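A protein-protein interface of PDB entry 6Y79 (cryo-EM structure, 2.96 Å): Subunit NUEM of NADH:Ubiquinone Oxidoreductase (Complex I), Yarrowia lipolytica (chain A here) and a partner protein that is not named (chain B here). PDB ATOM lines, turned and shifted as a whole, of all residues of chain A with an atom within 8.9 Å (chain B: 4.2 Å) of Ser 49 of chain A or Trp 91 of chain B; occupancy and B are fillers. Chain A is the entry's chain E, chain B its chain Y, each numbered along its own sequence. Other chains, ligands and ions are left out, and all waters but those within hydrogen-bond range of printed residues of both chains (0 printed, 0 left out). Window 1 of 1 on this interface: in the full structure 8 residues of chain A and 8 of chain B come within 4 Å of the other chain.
Printed residues of chain A that touch a printed residue of chain B: Lys 43, Gly 44, Thr 45, Ser 49 and Ser 50.
Of the 10 printed residues of chain B, 4 touch a printed residue of chain A.
Among the printed residues, 7 pairs touch across the chains.
O of Ala 88 of chain B lies within hydrogen-bond range of N of Gly 102 of chain B, at 3.3 Å.
The backbone carbonyl oxygen (O) of Trp 91 of chain B lies within hydrogen-bond range of the backbone NH (N) of Ser 100 of chain B (2.8 Å).
The backbone carbonyl oxygen (O) of Trp 98 of chain B lies within hydrogen-bond range of the backbone NH (N) of Asn 93 of chain B (3.0 Å).
The backbone NH of Lys 43 of chain A sits at hydrogen-bond distance from the backbone carbonyl oxygen of Arg 51 of chain A (3.0 Å).
OG of Ser 50 of chain A sits at hydrogen-bond distance from O of Thr 45 of chain A (2.5 Å).
O of Glu 92 of chain B sits at hydrogen-bond distance from NZ of Lys 43 of chain A, 2.6 Å away.
Of the printed residues of chain B, Ser 49 of chain A touches Trp 91 (3.99 Å).
Of the printed residues of chain A, Trp 91 of chain B touches Lys 43, Gly 44, Ser 49 and Ser 50.
No residue of chain A comes within 4 Å of Ser 100 of chain B.
Printed residues of chain B within 4 Å of Gly 44 of chain A: Trp 91 (3.5 Å).
Of the printed residues of chain A, Ala 88 of chain B touches Thr 45 (3.7 Å).
Gly 77 of chain A touches none of the printed residues of chain B.
His 76 of chain A touches none of the printed residues of chain B.
The nearest printed residue of chain A that does not touch Trp 91 of chain B is Thr 45 of chain A (4.1 Å).
Among the printed residues, pairs that only touch across the chains: Gly 44 of chain A with Trp 91 of chain B (3.5 Å), Thr 45 of chain A with Ala 88 of chain B (3.7 Å), Lys 43 of chain A with Trp 91 of chain B (3.8 Å), Lys 43 of chain A with Asn 93 of chain B (3.9 Å), Ser 50 of chain A with Trp 91 of chain B (3.98 Å) and Ser 49 of chain A with Trp 91 of chain B (3.99 Å).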
ATOM      1  N   MET A  21     -12.170 -14.569 -33.809  1.00  0.00           N
ATOM      2  CA  MET A  21     -12.101 -14.300 -32.379  1.00  0.00           C
ATOM      3  C   MET A  21     -11.888 -12.815 -32.122  1.00  0.00           C
ATOM      4  O   MET A  21     -11.854 -12.018 -33.057  1.00  0.00           O
ATOM      5  CB  MET A  21     -10.983 -15.116 -31.734  1.00  0.00           C
ATOM      6  CG  MET A  21      -9.597 -14.763 -32.221  1.00  0.00           C
ATOM      7  SD  MET A  21      -8.372 -15.981 -31.713  1.00  0.00           S
ATOM      8  CE  MET A  21      -6.909 -15.338 -32.513  1.00  0.00           C
ATOM      9  N   ASN A  22     -11.750 -12.447 -30.852  1.00  0.00           N
ATOM     10  CA  ASN A  22     -11.535 -11.058 -30.492  1.00  0.00           C
ATOM     11  C   ASN A  22     -10.111 -10.632 -30.840  1.00  0.00           C
ATOM     12  O   ASN A  22      -9.233 -11.454 -31.112  1.00  0.00           O
ATOM     13  CB  ASN A  22     -11.794 -10.843 -29.008  1.00  0.00           C
ATOM     14  CG  ASN A  22     -13.252 -10.956 -28.644  1.00  0.00           C
ATOM     15  OD1 ASN A  22     -14.125 -10.469 -29.359  1.00  0.00           O
ATOM     16  ND2 ASN A  22     -13.527 -11.599 -27.519  1.00  0.00           N
ATOM     17  N   PHE A  24      -7.176  -7.062 -30.264  1.00  0.00           N
ATOM     18  CA  PHE A  24      -6.818  -5.747 -29.749  1.00  0.00           C
ATOM     19  C   PHE A  24      -6.903  -4.700 -30.848  1.00  0.00           C
ATOM     20  O   PHE A  24      -5.946  -4.542 -31.613  1.00  0.00           O
ATOM     21  CB  PHE A  24      -5.394  -5.750 -29.199  1.00  0.00           C
ATOM     22  CG  PHE A  24      -5.202  -6.594 -27.984  1.00  0.00           C
ATOM     23  CD1 PHE A  24      -6.146  -6.623 -26.980  1.00  0.00           C
ATOM     24  CD2 PHE A  24      -4.058  -7.354 -27.845  1.00  0.00           C
ATOM     25  CE1 PHE A  24      -5.950  -7.402 -25.860  1.00  0.00           C
ATOM     26  CE2 PHE A  24      -3.860  -8.133 -26.733  1.00  0.00           C
ATOM     27  CZ  PHE A  24      -4.804  -8.154 -25.740  1.00  0.00           C
ATOM     28  N   ILE A  41       3.816  -6.041 -22.203  1.00  0.00           N
ATOM     29  CA  ILE A  41       3.494  -7.138 -23.103  1.00  0.00           C
ATOM     30  C   ILE A  41       2.017  -7.446 -22.926  1.00  0.00           C
ATOM     31  O   ILE A  41       1.592  -7.864 -21.847  1.00  0.00           O
ATOM     32  CB  ILE A  41       4.357  -8.370 -22.815  1.00  0.00           C
ATOM     33  CG1 ILE A  41       5.837  -8.034 -22.978  1.00  0.00           C
ATOM     34  CG2 ILE A  41       3.964  -9.505 -23.726  1.00  0.00           C
ATOM     35  CD1 ILE A  41       6.745  -9.116 -22.468  1.00  0.00           C
ATOM     36  N   ALA A  42       1.222  -7.230 -23.967  1.00  0.00           N
ATOM     37  CA  ALA A  42      -0.193  -7.551 -23.873  1.00  0.00           C
ATOM     38  C   ALA A  42      -0.391  -9.055 -23.980  1.00  0.00           C
ATOM     39  O   ALA A  42       0.378  -9.759 -24.634  1.00  0.00           O
ATOM     40  CB  ALA A  42      -0.987  -6.822 -24.953  1.00  0.00           C
ATOM     41  N   LYS A  43      -1.404  -9.560 -23.301  1.00  0.00           N
ATOM     42  CA  LYS A  43      -1.555 -10.994 -23.146  1.00  0.00           C
ATOM     43  C   LYS A  43      -2.846 -11.469 -23.785  1.00  0.00           C
ATOM     44  O   LYS A  43      -3.885 -10.827 -23.669  1.00  0.00           O
ATOM     45  CB  LYS A  43      -1.532 -11.376 -21.673  1.00  0.00           C
ATOM     46  CG  LYS A  43      -0.193 -11.146 -21.024  1.00  0.00           C
ATOM     47  CD  LYS A  43      -0.173 -11.740 -19.642  1.00  0.00           C
ATOM     48  CE  LYS A  43      -1.169 -11.036 -18.751  1.00  0.00           C
ATOM     49  NZ  LYS A  43      -1.090 -11.535 -17.360  1.00  0.00           N
ATOM     50  N   GLY A  44      -2.762 -12.586 -24.475  1.00  0.00           N
ATOM     51  CA  GLY A  44      -3.943 -13.215 -24.999  1.00  0.00           C
ATOM     52  C   GLY A  44      -4.524 -12.559 -26.233  1.00  0.00           C
ATOM     53  O   GLY A  44      -3.912 -11.731 -26.900  1.00  0.00           O
ATOM     54  N   THR A  45      -5.750 -12.970 -26.529  1.00  0.00           N
ATOM     55  CA  THR A  45      -6.529 -12.367 -27.597  1.00  0.00           C
ATOM     56  C   THR A  45      -7.167 -11.092 -27.061  1.00  0.00           C
ATOM     57  O   THR A  45      -6.896 -10.665 -25.940  1.00  0.00           O
ATOM     58  CB  THR A  45      -7.557 -13.358 -28.136  1.00  0.00           C
ATOM     59  OG1 THR A  45      -8.527 -13.648 -27.125  1.00  0.00           O
ATOM     60  CG2 THR A  45      -6.880 -14.649 -28.531  1.00  0.00           C
ATOM     61  N   GLY A  46      -8.014 -10.458 -27.836  1.00  0.00           N
ATOM     62  CA  GLY A  46      -8.716  -9.310 -27.312  1.00  0.00           C
ATOM     63  C   GLY A  46      -9.833  -9.724 -26.383  1.00  0.00           C
ATOM     64  O   GLY A  46     -10.131 -10.900 -26.198  1.00  0.00           O
ATOM     65  N   GLY A  47     -10.475  -8.742 -25.786  1.00  0.00           N
ATOM     66  CA  GLY A  47     -11.705  -9.008 -25.084  1.00  0.00           C
ATOM     67  C   GLY A  47     -11.584  -8.883 -23.580  1.00  0.00           C
ATOM     68  O   GLY A  47     -10.638  -8.305 -23.040  1.00  0.00           O
ATOM     69  N   ARG A  48     -12.573  -9.464 -22.896  1.00  0.00           N
ATOM     70  CA  ARG A  48     -12.805  -9.163 -21.487  1.00  0.00           C
ATOM     71  C   ARG A  48     -11.743  -9.786 -20.598  1.00  0.00           C
ATOM     72  O   ARG A  48     -11.176  -9.116 -19.730  1.00  0.00           O
ATOM     73  CB  ARG A  48     -14.191  -9.653 -21.080  1.00  0.00           C
ATOM     74  CG  ARG A  48     -14.531  -9.432 -19.628  1.00  0.00           C
ATOM     75  CD  ARG A  48     -15.977  -9.774 -19.364  1.00  0.00           C
ATOM     76  NE  ARG A  48     -16.375  -9.448 -18.001  1.00  0.00           N
ATOM     77  CZ  ARG A  48     -16.965  -8.314 -17.650  1.00  0.00           C
ATOM     78  NH1 ARG A  48     -17.291  -8.097 -16.388  1.00  0.00           N
ATOM     79  NH2 ARG A  48     -17.232  -7.399 -18.569  1.00  0.00           N
ATOM     80  N   SER A  49     -11.449 -11.058 -20.810  1.00  0.00           N
ATOM     81  CA  SER A  49     -10.599 -11.812 -19.903  1.00  0.00           C
ATOM     82  C   SER A  49      -9.107 -11.629 -20.149  1.00  0.00           C
ATOM     83  O   SER A  49      -8.313 -12.292 -19.479  1.00  0.00           O
ATOM     84  CB  SER A  49     -10.944 -13.292 -19.979  1.00  0.00           C
ATOM     85  OG  SER A  49      -9.982 -14.038 -19.271  1.00  0.00           O
ATOM     86  N   SER A  50      -8.698 -10.773 -21.076  1.00  0.00           N
ATOM     87  CA  SER A  50      -7.285 -10.518 -21.300  1.00  0.00           C
ATOM     88  C   SER A  50      -6.922  -9.088 -20.931  1.00  0.00           C
ATOM     89  O   SER A  50      -7.778  -8.257 -20.637  1.00  0.00           O
ATOM     90  CB  SER A  50      -6.914 -10.780 -22.745  1.00  0.00           C
ATOM     91  OG  SER A  50      -7.534  -9.855 -23.608  1.00  0.00           O
ATOM     92  N   ARG A  51      -5.620  -8.812 -20.959  1.00  0.00           N
ATOM     93  CA  ARG A  51      -5.064  -7.577 -20.430  1.00  0.00           C
ATOM     94  C   ARG A  51      -4.107  -6.960 -21.433  1.00  0.00           C
ATOM     95  O   ARG A  51      -3.271  -7.656 -22.010  1.00  0.00           O
ATOM     96  CB  ARG A  51      -4.316  -7.819 -19.120  1.00  0.00           C
ATOM     97  CG  ARG A  51      -5.125  -8.494 -18.050  1.00  0.00           C
ATOM     98  CD  ARG A  51      -6.275  -7.635 -17.638  1.00  0.00           C
ATOM     99  NE  ARG A  51      -6.894  -8.164 -16.427  1.00  0.00           N
ATOM    100  CZ  ARG A  51      -7.996  -8.900 -16.400  1.00  0.00           C
ATOM    101  NH1 ARG A  51      -8.459  -9.332 -15.247  1.00  0.00           N
ATOM    102  NH2 ARG A  51      -8.645  -9.178 -17.520  1.00  0.00           N
ATOM    103  N   THR A  52      -4.219  -5.647 -21.624  1.00  0.00           N
ATOM    104  CA  THR A  52      -3.295  -4.936 -22.501  1.00  0.00           C
ATOM    105  C   THR A  52      -2.001  -4.561 -21.794  1.00  0.00           C
ATOM    106  O   THR A  52      -0.925  -4.645 -22.392  1.00  0.00           O
ATOM    107  CB  THR A  52      -3.957  -3.677 -23.067  1.00  0.00           C
ATOM    108  OG1 THR A  52      -4.137  -2.717 -22.023  1.00  0.00           O
ATOM    109  CG2 THR A  52      -5.301  -4.013 -23.656  1.00  0.00           C
ATOM    110  N   ALA A  74     -11.733  -0.157 -20.386  1.00  0.00           N
ATOM    111  CA  ALA A  74     -11.763  -1.438 -19.693  1.00  0.00           C
ATOM    112  C   ALA A  74     -12.322  -2.564 -20.546  1.00  0.00           C
ATOM    113  O   ALA A  74     -12.443  -3.688 -20.054  1.00  0.00           O
ATOM    114  CB  ALA A  74     -12.587  -1.320 -18.411  1.00  0.00           C
ATOM    115  N   LYS A  75     -12.678  -2.283 -21.798  1.00  0.00           N
ATOM    116  CA  LYS A  75     -13.204  -3.307 -22.692  1.00  0.00           C
ATOM    117  C   LYS A  75     -12.126  -4.307 -23.082  1.00  0.00           C
ATOM    118  O   LYS A  75     -12.403  -5.501 -23.233  1.00  0.00           O
ATOM    119  CB  LYS A  75     -13.788  -2.627 -23.927  1.00  0.00           C
ATOM    120  CG  LYS A  75     -14.436  -3.510 -24.959  1.00  0.00           C
ATOM    121  CD  LYS A  75     -15.090  -2.611 -25.989  1.00  0.00           C
ATOM    122  CE  LYS A  75     -15.753  -3.371 -27.111  1.00  0.00           C
ATOM    123  NZ  LYS A  75     -16.397  -2.417 -28.061  1.00  0.00           N
ATOM    124  N   HIS A  76     -10.890  -3.840 -23.229  1.00  0.00           N
ATOM    125  CA  HIS A  76      -9.786  -4.673 -23.673  1.00  0.00           C
ATOM    126  C   HIS A  76      -8.871  -5.113 -22.553  1.00  0.00           C
ATOM    127  O   HIS A  76      -7.937  -5.875 -22.805  1.00  0.00           O
ATOM    128  CB  HIS A  76      -8.977  -3.936 -24.731  1.00  0.00           C
ATOM    129  CG  HIS A  76      -9.733  -3.751 -25.994  1.00  0.00           C
ATOM    130  ND1 HIS A  76     -10.080  -4.813 -26.796  1.00  0.00           N
ATOM    131  CD2 HIS A  76     -10.257  -2.649 -26.575  1.00  0.00           C
ATOM    132  CE1 HIS A  76     -10.772  -4.373 -27.827  1.00  0.00           C
ATOM    133  NE2 HIS A  76     -10.890  -3.063 -27.720  1.00  0.00           N
ATOM    134  N   GLY A  77      -9.111  -4.660 -21.334  1.00  0.00           N
ATOM    135  CA  GLY A  77      -8.316  -5.077 -20.212  1.00  0.00           C
ATOM    136  C   GLY A  77      -7.288  -4.086 -19.742  1.00  0.00           C
ATOM    137  O   GLY A  77      -6.345  -4.486 -19.056  1.00  0.00           O
ATOM    138  N   THR A  96     -18.303  -2.830 -16.491  1.00  0.00           N
ATOM    139  CA  THR A  96     -17.608  -2.598 -17.751  1.00  0.00           C
ATOM    140  C   THR A  96     -16.321  -3.384 -17.911  1.00  0.00           C
ATOM    141  O   THR A  96     -15.908  -3.636 -19.047  1.00  0.00           O
ATOM    142  CB  THR A  96     -17.257  -1.119 -17.896  1.00  0.00           C
ATOM    143  OG1 THR A  96     -16.071  -0.842 -17.144  1.00  0.00           O
ATOM    144  CG2 THR A  96     -18.373  -0.274 -17.377  1.00  0.00           C
ATOM    145  N   GLY A  97     -15.659  -3.759 -16.818  1.00  0.00           N
ATOM    146  CA  GLY A  97     -14.360  -4.378 -16.889  1.00  0.00           C
ATOM    147  C   GLY A  97     -14.371  -5.776 -16.297  1.00  0.00           C
ATOM    148  O   GLY A  97     -15.326  -6.199 -15.640  1.00  0.00           O
ATOM    149  N   ASP A  98     -13.279  -6.488 -16.540  1.00  0.00           N
ATOM    150  CA  ASP A  98     -13.056  -7.784 -15.927  1.00  0.00           C
ATOM    151  C   ASP A  98     -12.889  -7.645 -14.418  1.00  0.00           C
ATOM    152  O   ASP A  98     -12.701  -6.551 -13.875  1.00  0.00           O
ATOM    153  CB  ASP A  98     -11.817  -8.442 -16.534  1.00  0.00           C
ATOM    154  CG  ASP A  98     -11.796  -9.948 -16.362  1.00  0.00           C
ATOM    155  OD1 ASP A  98     -12.857 -10.540 -16.073  1.00  0.00           O
ATOM    156  OD2 ASP A  98     -10.704 -10.538 -16.503  1.00  0.00           O
ATOM    157  N   LEU A  99     -13.009  -8.775 -13.741  1.00  0.00           N
ATOM    158  CA  LEU A  99     -12.653  -8.898 -12.338  1.00  0.00           C
ATOM    159  C   LEU A  99     -11.190  -8.526 -12.125  1.00  0.00           C
ATOM    160  O   LEU A  99     -10.290  -9.209 -12.614  1.00  0.00           O
ATOM    161  CB  LEU A  99     -12.937 -10.340 -11.917  1.00  0.00           C
ATOM    162  CG  LEU A  99     -12.784 -10.938 -10.527  1.00  0.00           C
ATOM    163  CD1 LEU A  99     -13.670 -12.070 -10.409  1.00  0.00           C
ATOM    164  CD2 LEU A  99     -11.475 -11.543 -10.466  1.00  0.00           C
ATOM    165  N   VAL A 101     -10.045  -5.320 -12.983  1.00  0.00           N
ATOM    166  CA  VAL A 101      -9.627  -4.312 -13.955  1.00  0.00           C
ATOM    167  C   VAL A 101      -9.886  -2.904 -13.427  1.00  0.00           C
ATOM    168  O   VAL A 101      -8.963  -2.087 -13.338  1.00  0.00           O
ATOM    169  CB  VAL A 101     -10.301  -4.570 -15.317  1.00  0.00           C
ATOM    170  CG1 VAL A 101     -10.376  -3.320 -16.164  1.00  0.00           C
ATOM    171  CG2 VAL A 101      -9.506  -5.592 -16.064  1.00  0.00           C
ATOM    172  N   ALA B  88      -3.411 -17.666 -28.556  1.00  0.00           N
ATOM    173  CA  ALA B  88      -4.623 -17.944 -27.806  1.00  0.00           C
ATOM    174  C   ALA B  88      -4.502 -19.132 -26.872  1.00  0.00           C
ATOM    175  O   ALA B  88      -5.499 -19.468 -26.230  1.00  0.00           O
ATOM    176  CB  ALA B  88      -5.797 -18.189 -28.757  1.00  0.00           C
ATOM    177  N   ARG B  90      -2.553 -20.215 -23.846  1.00  0.00           N
ATOM    178  CA  ARG B  90      -2.652 -20.013 -22.404  1.00  0.00           C
ATOM    179  C   ARG B  90      -1.785 -18.837 -21.983  1.00  0.00           C
ATOM    180  O   ARG B  90      -0.713 -18.604 -22.546  1.00  0.00           O
ATOM    181  CB  ARG B  90      -2.222 -21.241 -21.586  1.00  0.00           C
ATOM    182  CG  ARG B  90      -3.247 -22.339 -21.444  1.00  0.00           C
ATOM    183  CD  ARG B  90      -2.690 -23.507 -20.738  1.00  0.00           C
ATOM    184  NE  ARG B  90      -3.447 -24.721 -20.994  1.00  0.00           N
ATOM    185  CZ  ARG B  90      -4.496 -25.094 -20.285  1.00  0.00           C
ATOM    186  NH1 ARG B  90      -4.879 -24.357 -19.257  1.00  0.00           N
ATOM    187  NH2 ARG B  90      -5.143 -26.209 -20.587  1.00  0.00           N
ATOM    188  N   TRP B  91      -2.257 -18.107 -20.973  1.00  0.00           N
ATOM    189  CA  TRP B  91      -1.457 -17.074 -20.330  1.00  0.00           C
ATOM    190  C   TRP B  91      -1.841 -16.980 -18.864  1.00  0.00           C
ATOM    191  O   TRP B  91      -2.961 -17.315 -18.481  1.00  0.00           O
ATOM    192  CB  TRP B  91      -1.621 -15.706 -21.000  1.00  0.00           C
ATOM    193  CG  TRP B  91      -3.004 -15.144 -20.985  1.00  0.00           C
ATOM    194  CD1 TRP B  91      -3.516 -14.260 -20.093  1.00  0.00           C
ATOM    195  CD2 TRP B  91      -4.039 -15.406 -21.930  1.00  0.00           C
ATOM    196  NE1 TRP B  91      -4.812 -13.963 -20.414  1.00  0.00           N
ATOM    197  CE2 TRP B  91      -5.158 -14.659 -21.539  1.00  0.00           C
ATOM    198  CE3 TRP B  91      -4.134 -16.215 -23.060  1.00  0.00           C
ATOM    199  CZ2 TRP B  91      -6.349 -14.691 -22.240  1.00  0.00           C
ATOM    200  CZ3 TRP B  91      -5.316 -16.242 -23.753  1.00  0.00           C
ATOM    201  CH2 TRP B  91      -6.407 -15.482 -23.346  1.00  0.00           C
ATOM    202  N   GLU B  92      -0.899 -16.515 -18.046  1.00  0.00           N
ATOM    203  CA  GLU B  92      -1.124 -16.427 -16.610  1.00  0.00           C
ATOM    204  C   GLU B  92      -1.812 -15.121 -16.245  1.00  0.00           C
ATOM    205  O   GLU B  92      -1.565 -14.080 -16.854  1.00  0.00           O
ATOM    206  CB  GLU B  92       0.188 -16.552 -15.848  1.00  0.00           C
ATOM    207  CG  GLU B  92       1.355 -15.859 -16.502  1.00  0.00           C
ATOM    208  CD  GLU B  92       2.666 -16.290 -15.892  1.00  0.00           C
ATOM    209  OE1 GLU B  92       2.622 -16.951 -14.840  1.00  0.00           O
ATOM    210  OE2 GLU B  92       3.729 -15.971 -16.462  1.00  0.00           O
ATOM    211  N   ASN B  93      -2.662 -15.184 -15.232  1.00  0.00           N
ATOM    212  CA  ASN B  93      -3.531 -14.071 -14.891  1.00  0.00           C
ATOM    213  C   ASN B  93      -2.760 -12.987 -14.148  1.00  0.00           C
ATOM    214  O   ASN B  93      -1.767 -13.271 -13.470  1.00  0.00           O
ATOM    215  CB  ASN B  93      -4.697 -14.580 -14.038  1.00  0.00           C
ATOM    216  CG  ASN B  93      -5.801 -13.557 -13.860  1.00  0.00           C
ATOM    217  OD1 ASN B  93      -5.762 -12.461 -14.416  1.00  0.00           O
ATOM    218  ND2 ASN B  93      -6.800 -13.918 -13.072  1.00  0.00           N
ATOM    219  N   TRP B  98      -4.030 -17.682 -12.415  1.00  0.00           N
ATOM    220  CA  TRP B  98      -4.800 -18.702 -13.093  1.00  0.00           C
ATOM    221  C   TRP B  98      -4.371 -18.794 -14.544  1.00  0.00           C
ATOM    222  O   TRP B  98      -4.067 -17.789 -15.184  1.00  0.00           O
ATOM    223  CB  TRP B  98      -6.281 -18.378 -13.030  1.00  0.00           C
ATOM    224  CG  TRP B  98      -6.885 -18.560 -11.706  1.00  0.00           C
ATOM    225  CD1 TRP B  98      -6.332 -19.168 -10.626  1.00  0.00           C
ATOM    226  CD2 TRP B  98      -8.178 -18.128 -11.311  1.00  0.00           C
ATOM    227  NE1 TRP B  98      -7.208 -19.139  -9.576  1.00  0.00           N
ATOM    228  CE2 TRP B  98      -8.352 -18.505  -9.976  1.00  0.00           C
ATOM    229  CE3 TRP B  98      -9.210 -17.453 -11.961  1.00  0.00           C
ATOM    230  CZ2 TRP B  98      -9.514 -18.232  -9.278  1.00  0.00           C
ATOM    231  CZ3 TRP B  98     -10.356 -17.184 -11.272  1.00  0.00           C
ATOM    232  CH2 TRP B  98     -10.503 -17.571  -9.945  1.00  0.00           C
ATOM    233  N   GLN B  99      -4.336 -20.009 -15.054  1.00  0.00           N
ATOM    234  CA  GLN B  99      -4.081 -20.239 -16.464  1.00  0.00           C
ATOM    235  C   GLN B  99      -5.336 -19.870 -17.239  1.00  0.00           C
ATOM    236  O   GLN B  99      -6.315 -20.612 -17.239  1.00  0.00           O
ATOM    237  CB  GLN B  99      -3.695 -21.692 -16.671  1.00  0.00           C
ATOM    238  CG  GLN B  99      -2.505 -22.088 -15.850  1.00  0.00           C
ATOM    239  CD  GLN B  99      -1.270 -21.469 -16.392  1.00  0.00           C
ATOM    240  OE1 GLN B  99      -1.118 -21.366 -17.600  1.00  0.00           O
ATOM    241  NE2 GLN B  99      -0.374 -21.052 -15.518  1.00  0.00           N
ATOM    242  N   SER B 100      -5.314 -18.711 -17.887  1.00  0.00           N
ATOM    243  CA  SER B 100      -6.419 -18.217 -18.695  1.00  0.00           C
ATOM    244  C   SER B 100      -6.202 -18.605 -20.147  1.00  0.00           C
ATOM    245  O   SER B 100      -5.069 -18.743 -20.596  1.00  0.00           O
ATOM    246  CB  SER B 100      -6.532 -16.702 -18.601  1.00  0.00           C
ATOM    247  OG  SER B 100      -6.736 -16.293 -17.270  1.00  0.00           O
ATOM    248  N   SER B 101      -7.287 -18.775 -20.889  1.00  0.00           N
ATOM    249  CA  SER B 101      -7.174 -19.194 -22.275  1.00  0.00           C
ATOM    250  C   SER B 101      -8.286 -18.587 -23.118  1.00  0.00           C
ATOM    251  O   SER B 101      -9.401 -18.358 -22.652  1.00  0.00           O
ATOM    252  CB  SER B 101      -7.212 -20.717 -22.407  1.00  0.00           C
ATOM    253  OG  SER B 101      -8.511 -21.239 -22.270  1.00  0.00           O
ATOM    254  N   GLY B 102      -7.970 -18.357 -24.386  1.00  0.00           N
ATOM    255  CA  GLY B 102      -8.952 -17.930 -25.359  1.00  0.00           C
ATOM    256  C   GLY B 102      -9.214 -19.009 -26.385  1.00  0.00           C
ATOM    257  O   GLY B 102     -10.207 -18.961 -27.112  1.00  0.00           O
